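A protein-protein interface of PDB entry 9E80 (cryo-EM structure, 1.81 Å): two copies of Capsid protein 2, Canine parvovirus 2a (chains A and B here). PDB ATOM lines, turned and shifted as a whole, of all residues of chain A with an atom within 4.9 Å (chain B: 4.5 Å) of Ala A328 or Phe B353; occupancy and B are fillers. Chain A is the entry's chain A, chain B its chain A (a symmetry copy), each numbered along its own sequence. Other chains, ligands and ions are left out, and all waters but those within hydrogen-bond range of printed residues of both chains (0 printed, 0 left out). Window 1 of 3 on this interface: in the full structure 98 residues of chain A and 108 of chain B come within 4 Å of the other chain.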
ATOM      1  N   THR A 281       6.464  35.681 -26.225  1.00  0.00           N
ATOM      2  CA  THR A 281       5.687  35.424 -25.026  1.00  0.00           C
ATOM      3  C   THR A 281       6.550  34.642 -24.038  1.00  0.00           C
ATOM      4  O   THR A 281       7.738  34.403 -24.269  1.00  0.00           O
ATOM      5  CB  THR A 281       4.406  34.665 -25.367  1.00  0.00           C
ATOM      6  OG1 THR A 281       4.729  33.313 -25.715  1.00  0.00           O
ATOM      7  CG2 THR A 281       3.681  35.330 -26.530  1.00  0.00           C
ATOM      8  N   ASN A 282       5.948  34.223 -22.923  1.00  0.00           N
ATOM      9  CA  ASN A 282       6.692  33.442 -21.939  1.00  0.00           C
ATOM     10  C   ASN A 282       7.259  32.170 -22.557  1.00  0.00           C
ATOM     11  O   ASN A 282       8.302  31.670 -22.121  1.00  0.00           O
ATOM     12  CB  ASN A 282       5.791  33.096 -20.754  1.00  0.00           C
ATOM     13  CG  ASN A 282       5.978  34.044 -19.591  1.00  0.00           C
ATOM     14  OD1 ASN A 282       5.866  35.256 -19.748  1.00  0.00           O
ATOM     15  ND2 ASN A 282       6.271  33.495 -18.417  1.00  0.00           N
ATOM     16  N   ARG A 283       6.589  31.639 -23.580  1.00  0.00           N
ATOM     17  CA  ARG A 283       7.007  30.373 -24.169  1.00  0.00           C
ATOM     18  C   ARG A 283       8.282  30.504 -24.993  1.00  0.00           C
ATOM     19  O   ARG A 283       8.917  29.487 -25.291  1.00  0.00           O
ATOM     20  CB  ARG A 283       5.883  29.811 -25.041  1.00  0.00           C
ATOM     21  CG  ARG A 283       4.774  29.113 -24.267  1.00  0.00           C
ATOM     22  CD  ARG A 283       5.223  27.765 -23.718  1.00  0.00           C
ATOM     23  NE  ARG A 283       5.397  26.770 -24.771  1.00  0.00           N
ATOM     24  CZ  ARG A 283       4.473  25.893 -25.145  1.00  0.00           C
ATOM     25  NH1 ARG A 283       3.274  25.868 -24.586  1.00  0.00           N
ATOM     26  NH2 ARG A 283       4.760  25.019 -26.105  1.00  0.00           N
ATOM     27  N   THR A 326       8.441  20.833 -18.867  1.00  0.00           N
ATOM     28  CA  THR A 326       7.920  21.030 -20.208  1.00  0.00           C
ATOM     29  C   THR A 326       8.010  22.509 -20.554  1.00  0.00           C
ATOM     30  O   THR A 326       8.265  23.356 -19.694  1.00  0.00           O
ATOM     31  CB  THR A 326       6.469  20.541 -20.322  1.00  0.00           C
ATOM     32  OG1 THR A 326       5.596  21.460 -19.655  1.00  0.00           O
ATOM     33  CG2 THR A 326       6.320  19.158 -19.698  1.00  0.00           C
ATOM     34  N   GLU A 327       7.808  22.818 -21.834  1.00  0.00           N
ATOM     35  CA  GLU A 327       7.811  24.216 -22.244  1.00  0.00           C
ATOM     36  C   GLU A 327       6.751  25.011 -21.495  1.00  0.00           C
ATOM     37  O   GLU A 327       6.922  26.213 -21.265  1.00  0.00           O
ATOM     38  CB  GLU A 327       7.591  24.320 -23.753  1.00  0.00           C
ATOM     39  CG  GLU A 327       8.789  23.871 -24.572  1.00  0.00           C
ATOM     40  CD  GLU A 327      10.030  24.698 -24.287  1.00  0.00           C
ATOM     41  OE1 GLU A 327      10.139  25.822 -24.821  1.00  0.00           O
ATOM     42  OE2 GLU A 327      10.886  24.230 -23.510  1.00  0.00           O
ATOM     43  N   ALA A 328       5.656  24.359 -21.103  1.00  0.00           N
ATOM     44  CA  ALA A 328       4.610  25.038 -20.349  1.00  0.00           C
ATOM     45  C   ALA A 328       4.984  25.235 -18.885  1.00  0.00           C
ATOM     46  O   ALA A 328       4.551  26.215 -18.269  1.00  0.00           O
ATOM     47  CB  ALA A 328       3.302  24.252 -20.450  1.00  0.00           C
ATOM     48  N   THR A 329       5.777  24.326 -18.312  1.00  0.00           N
ATOM     49  CA  THR A 329       6.068  24.352 -16.882  1.00  0.00           C
ATOM     50  C   THR A 329       7.465  24.853 -16.546  1.00  0.00           C
ATOM     51  O   THR A 329       7.731  25.141 -15.374  1.00  0.00           O
ATOM     52  CB  THR A 329       5.899  22.952 -16.277  1.00  0.00           C
ATOM     53  OG1 THR A 329       6.885  22.069 -16.827  1.00  0.00           O
ATOM     54  CG2 THR A 329       4.507  22.402 -16.560  1.00  0.00           C
ATOM     55  N   ILE A 330       8.365  24.960 -17.526  1.00  0.00           N
ATOM     56  CA  ILE A 330       9.722  25.394 -17.226  1.00  0.00           C
ATOM     57  C   ILE A 330       9.697  26.828 -16.718  1.00  0.00           C
ATOM     58  O   ILE A 330       8.887  27.655 -17.157  1.00  0.00           O
ATOM     59  CB  ILE A 330      10.628  25.255 -18.460  1.00  0.00           C
ATOM     60  CG1 ILE A 330      12.100  25.300 -18.036  1.00  0.00           C
ATOM     61  CG2 ILE A 330      10.322  26.344 -19.481  1.00  0.00           C
ATOM     62  CD1 ILE A 330      13.059  24.767 -19.077  1.00  0.00           C
ATOM     63  N   GLU A 335       6.766  37.296 -16.361  1.00  0.00           N
ATOM     64  CA  GLU A 335       5.566  37.126 -17.172  1.00  0.00           C
ATOM     65  C   GLU A 335       5.464  38.268 -18.170  1.00  0.00           C
ATOM     66  O   GLU A 335       5.534  39.441 -17.787  1.00  0.00           O
ATOM     67  CB  GLU A 335       4.311  37.071 -16.301  1.00  0.00           C
ATOM     68  CG  GLU A 335       3.068  36.663 -17.079  1.00  0.00           C
ATOM     69  CD  GLU A 335       1.911  36.267 -16.185  1.00  0.00           C
ATOM     70  OE1 GLU A 335       2.158  35.864 -15.029  1.00  0.00           O
ATOM     71  OE2 GLU A 335       0.753  36.350 -16.644  1.00  0.00           O
ATOM     72  N   VAL A 336       5.289  37.925 -19.441  1.00  0.00           N
ATOM     73  CA  VAL A 336       5.042  38.913 -20.485  1.00  0.00           C
ATOM     74  C   VAL A 336       3.535  39.079 -20.623  1.00  0.00           C
ATOM     75  O   VAL A 336       2.820  38.113 -20.907  1.00  0.00           O
ATOM     76  CB  VAL A 336       5.675  38.493 -21.818  1.00  0.00           C
ATOM     77  CG1 VAL A 336       5.355  39.517 -22.900  1.00  0.00           C
ATOM     78  CG2 VAL A 336       7.181  38.320 -21.667  1.00  0.00           C
ATOM     79  N   ARG A 408      -3.466  38.131 -24.449  1.00  0.00           N
ATOM     80  CA  ARG A 408      -3.841  36.835 -23.908  1.00  0.00           C
ATOM     81  C   ARG A 408      -4.900  36.188 -24.787  1.00  0.00           C
ATOM     82  O   ARG A 408      -5.695  36.870 -25.441  1.00  0.00           O
ATOM     83  CB  ARG A 408      -4.370  36.962 -22.473  1.00  0.00           C
ATOM     84  CG  ARG A 408      -3.294  37.265 -21.447  1.00  0.00           C
ATOM     85  CD  ARG A 408      -2.434  36.043 -21.171  1.00  0.00           C
ATOM     86  NE  ARG A 408      -1.429  36.305 -20.148  1.00  0.00           N
ATOM     87  CZ  ARG A 408      -0.249  36.864 -20.378  1.00  0.00           C
ATOM     88  NH1 ARG A 408       0.113  37.245 -21.593  1.00  0.00           N
ATOM     89  NH2 ARG A 408       0.590  37.047 -19.362  1.00  0.00           N
ATOM     90  N   ALA B  97      -0.774  20.642 -19.885  1.00  0.00           N
ATOM     91  CA  ALA B  97       0.411  21.144 -19.197  1.00  0.00           C
ATOM     92  C   ALA B  97       1.693  20.520 -19.732  1.00  0.00           C
ATOM     93  O   ALA B  97       2.780  21.047 -19.471  1.00  0.00           O
ATOM     94  CB  ALA B  97       0.298  20.889 -17.694  1.00  0.00           C
ATOM     95  N   ASP B  99       2.616  20.345 -22.843  1.00  0.00           N
ATOM     96  CA  ASP B  99       2.942  20.853 -24.168  1.00  0.00           C
ATOM     97  C   ASP B  99       4.429  21.163 -24.270  1.00  0.00           C
ATOM     98  O   ASP B  99       5.002  21.820 -23.397  1.00  0.00           O
ATOM     99  CB  ASP B  99       2.123  22.109 -24.467  1.00  0.00           C
ATOM    100  CG  ASP B  99       2.285  22.582 -25.898  1.00  0.00           C
ATOM    101  OD1 ASP B  99       2.587  21.745 -26.771  1.00  0.00           O
ATOM    102  OD2 ASP B  99       2.114  23.794 -26.147  1.00  0.00           O
ATOM    103  N   SER B 344      -2.152  28.189 -12.312  1.00  0.00           N
ATOM    104  CA  SER B 344      -2.920  28.788 -13.391  1.00  0.00           C
ATOM    105  C   SER B 344      -2.065  28.811 -14.649  1.00  0.00           C
ATOM    106  O   SER B 344      -0.884  29.167 -14.599  1.00  0.00           O
ATOM    107  CB  SER B 344      -3.353  30.203 -13.014  1.00  0.00           C
ATOM    108  OG  SER B 344      -3.504  31.017 -14.163  1.00  0.00           O
ATOM    109  N   PHE B 345      -2.655  28.420 -15.772  1.00  0.00           N
ATOM    110  CA  PHE B 345      -1.967  28.407 -17.055  1.00  0.00           C
ATOM    111  C   PHE B 345      -2.626  29.425 -17.974  1.00  0.00           C
ATOM    112  O   PHE B 345      -3.808  29.292 -18.308  1.00  0.00           O
ATOM    113  CB  PHE B 345      -1.990  27.009 -17.672  1.00  0.00           C
ATOM    114  CG  PHE B 345      -1.019  26.057 -17.034  1.00  0.00           C
ATOM    115  CD1 PHE B 345      -1.367  25.352 -15.896  1.00  0.00           C
ATOM    116  CD2 PHE B 345       0.248  25.876 -17.567  1.00  0.00           C
ATOM    117  CE1 PHE B 345      -0.474  24.481 -15.302  1.00  0.00           C
ATOM    118  CE2 PHE B 345       1.145  25.008 -16.979  1.00  0.00           C
ATOM    119  CZ  PHE B 345       0.783  24.311 -15.845  1.00  0.00           C
ATOM    120  N   GLU B 346      -1.864  30.440 -18.364  1.00  0.00           N
ATOM    121  CA  GLU B 346      -2.322  31.458 -19.295  1.00  0.00           C
ATOM    122  C   GLU B 346      -1.831  31.126 -20.696  1.00  0.00           C
ATOM    123  O   GLU B 346      -0.776  30.513 -20.876  1.00  0.00           O
ATOM    124  CB  GLU B 346      -1.823  32.845 -18.887  1.00  0.00           C
ATOM    125  CG  GLU B 346      -2.366  33.336 -17.555  1.00  0.00           C
ATOM    126  CD  GLU B 346      -1.734  34.646 -17.119  1.00  0.00           C
ATOM    127  OE1 GLU B 346      -2.119  35.700 -17.663  1.00  0.00           O
ATOM    128  OE2 GLU B 346      -0.855  34.619 -16.232  1.00  0.00           O
ATOM    129  N   ALA B 347      -2.610  31.535 -21.690  1.00  0.00           N
ATOM    130  CA  ALA B 347      -2.307  31.256 -23.083  1.00  0.00           C
ATOM    131  C   ALA B 347      -2.057  32.556 -23.832  1.00  0.00           C
ATOM    132  O   ALA B 347      -2.706  33.576 -23.584  1.00  0.00           O
ATOM    133  CB  ALA B 347      -3.442  30.478 -23.757  1.00  0.00           C
ATOM    134  N   SER B 348      -1.098  32.499 -24.750  1.00  0.00           N
ATOM    135  CA  SER B 348      -0.786  33.616 -25.626  1.00  0.00           C
ATOM    136  C   SER B 348      -0.494  33.063 -27.014  1.00  0.00           C
ATOM    137  O   SER B 348      -0.861  31.924 -27.319  1.00  0.00           O
ATOM    138  CB  SER B 348       0.392  34.428 -25.086  1.00  0.00           C
ATOM    139  OG  SER B 348       0.444  35.708 -25.694  1.00  0.00           O
ATOM    140  N   GLY B 351       1.079  29.510 -27.100  1.00  0.00           N
ATOM    141  CA  GLY B 351       0.519  28.421 -26.336  1.00  0.00           C
ATOM    142  C   GLY B 351       0.590  28.669 -24.841  1.00  0.00           C
ATOM    143  O   GLY B 351       1.074  29.709 -24.382  1.00  0.00           O
ATOM    144  N   PRO B 352       0.118  27.707 -24.052  1.00  0.00           N
ATOM    145  CA  PRO B 352      -0.020  27.931 -22.610  1.00  0.00           C
ATOM    146  C   PRO B 352       1.310  27.919 -21.875  1.00  0.00           C
ATOM    147  O   PRO B 352       2.262  27.238 -22.258  1.00  0.00           O
ATOM    148  CB  PRO B 352      -0.903  26.761 -22.162  1.00  0.00           C
ATOM    149  CG  PRO B 352      -0.564  25.663 -23.115  1.00  0.00           C
ATOM    150  CD  PRO B 352      -0.244  26.331 -24.436  1.00  0.00           C
ATOM    151  N   PHE B 353       1.354  28.694 -20.793  1.00  0.00           N
ATOM    152  CA  PHE B 353       2.507  28.748 -19.909  1.00  0.00           C
ATOM    153  C   PHE B 353       2.026  28.983 -18.485  1.00  0.00           C
ATOM    154  O   PHE B 353       1.018  29.655 -18.258  1.00  0.00           O
ATOM    155  CB  PHE B 353       3.484  29.856 -20.321  1.00  0.00           C
ATOM    156  CG  PHE B 353       2.843  31.208 -20.445  1.00  0.00           C
ATOM    157  CD1 PHE B 353       2.718  32.035 -19.341  1.00  0.00           C
ATOM    158  CD2 PHE B 353       2.359  31.648 -21.665  1.00  0.00           C
ATOM    159  CE1 PHE B 353       2.125  33.276 -19.453  1.00  0.00           C
ATOM    160  CE2 PHE B 353       1.766  32.889 -21.782  1.00  0.00           C
ATOM    161  CZ  PHE B 353       1.651  33.705 -20.674  1.00  0.00           C
ATOM    162  N   LYS B 354       2.758  28.424 -17.525  1.00  0.00           N
ATOM    163  CA  LYS B 354       2.396  28.584 -16.123  1.00  0.00           C
ATOM    164  C   LYS B 354       2.594  30.030 -15.690  1.00  0.00           C
ATOM    165  O   LYS B 354       3.594  30.663 -16.039  1.00  0.00           O
ATOM    166  CB  LYS B 354       3.234  27.660 -15.244  1.00  0.00           C
ATOM    167  CG  LYS B 354       2.653  27.460 -13.851  1.00  0.00           C
ATOM    168  CD  LYS B 354       3.648  26.806 -12.909  1.00  0.00           C
ATOM    169  CE  LYS B 354       4.604  27.827 -12.316  1.00  0.00           C
ATOM    170  NZ  LYS B 354       3.948  28.662 -11.270  1.00  0.00           N
ATOM    171  N   THR B 355       1.644  30.548 -14.924  1.00  0.00           N
ATOM    172  CA  THR B 355       1.773  31.888 -14.374  1.00  0.00           C
ATOM    173  C   THR B 355       2.800  31.875 -13.244  1.00  0.00           C
ATOM    174  O   THR B 355       2.590  31.173 -12.244  1.00  0.00           O
ATOM    175  CB  THR B 355       0.427  32.387 -13.850  1.00  0.00           C
ATOM    176  OG1 THR B 355      -0.553  32.332 -14.895  1.00  0.00           O
ATOM    177  CG2 THR B 355       0.543  33.817 -13.339  1.00  0.00           C
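Hydrophobic or aromatic side chains of chain B within 4 Å of the printed part of chain A: Phe B345, Pro B352 and Phe B353.
Printed residues of chain A that touch a printed residue of chain B: Thr A281, Asn A282, Arg A283, Thr A326, Glu A327, Ala A328, Thr A329, Glu A335 and Arg A408.
Hydrophobic or aromatic side chains of chain A that line the printed part of chain B: Ala A328.
Among the printed residues, Asp or Glu carboxylates within 4 Å of a Lys or Arg side-chain nitrogen of the other chain: Arg A283 with Asp B99 (2.8 Å) and Arg A408 with Glu B346 (2.6 Å).
The side-chain amide oxygen (OD1) of Asn A282 sits at hydrogen-bond distance from the backbone NH (N) of Val A336.
OG1 of Thr A326 lies close to N of Ala A328 (3.2 Å).
The guanidinium group (NH2) of Arg A408 lies within salt-bridge range of the side-chain carboxylate (OE2) of Glu A335, 2.8 Å away.
The backbone carbonyl oxygen (O) of Val A336 lies within hydrogen-bond range of the guanidinium group (NH2) of Arg A408, at 2.9 Å.
The backbone carbonyl oxygen of Ser B344 lies within hydrogen-bond range of the backbone NH of Thr B355 (2.9 Å).
The side-chain hydroxyl (OG1) of Thr B355 lies within hydrogen-bond range of the side-chain carboxylate (OE2) of Glu B346, at 2.7 Å.
Thr A281 touches Ser B348 (CG2 to OG, 3.4 Å).
CG of Arg A283 touches O of Gly B351, at 3.7 Å.
Thr A326 touches Asp B99 (CB to O, 3.6 Å).
O of Ala A328 touches CE2 of Phe B345 (3.8 Å).
Pro B352 touches Ala A328 (O to CB, 3.6 Å).
Phe B353 touches Ala A328.
Thr A329 touches Ala B97.
Glu A335 touches Thr B355 (OE1 to CG2, 3.1 Å).
Ala B347 touches Arg A408 (O to CD, 3.5 Å).
CZ of Arg A408 touches CZ of Phe B353, 3.7 Å away.
Of the printed residues of chain B, Ala A328 touches Ala B97 (3.4 Å), Asp B99 (3.5 Å), Phe B345 (3.8 Å), Pro B352 (3.6 Å), Phe B353 (3.6 Å) and Lys B354 (2.9 Å).
Phe B353 touches just these residues of chain A: Asn A282, Ala A328 and Arg A408.
Printed residues of chain A within 4 Å of Lys B354: Ala A328.
Of the printed residues of chain A, Ala B97 touches Thr A326 (2.9 Å), Ala A328 (3.4 Å) and Thr A329 (3.6 Å).
Printed residues of chain B within 4 Å of Glu A335: Glu B346 (2.4 Å) and Thr B355 (3.1 Å).
Ser B344 touches none of the printed residues of chain A.
The nearest printed residue of chain A that does not touch Thr B355 is Ala A328 (6.2 Å).
The side-chain carboxylate (OD2) of Asp B99 lies within salt-bridge range of the guanidinium group (NH1) of Arg A283 (2.8 Å).
NH1 of Arg A283 sits at hydrogen-bond distance from O of Pro B352 (2.9 Å).
The side-chain hydroxyl (OG1) of Thr A326 sits at hydrogen-bond distance from the backbone carbonyl oxygen (O) of Ala B97, at 2.9 Å.
O of Asp B99 sits at hydrogen-bond distance from N of Glu A327 (3.4 Å).
O of Asp B99 is in hydrogen-bond range of N of Ala A328.
O of Ala A328 is in hydrogen-bond range of N of Lys B354.
NE of Arg A408 lies within salt-bridge range of OE1 of Glu B346 (2.6 Å).
The side-chain carboxylate of Glu A335 lies close to the side-chain carboxylate of Glu B346.
No position is printed for both chains.
Of the 20 pairs that touch across the chains among the printed residues, none has its exchanged pair printed and touching as well.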
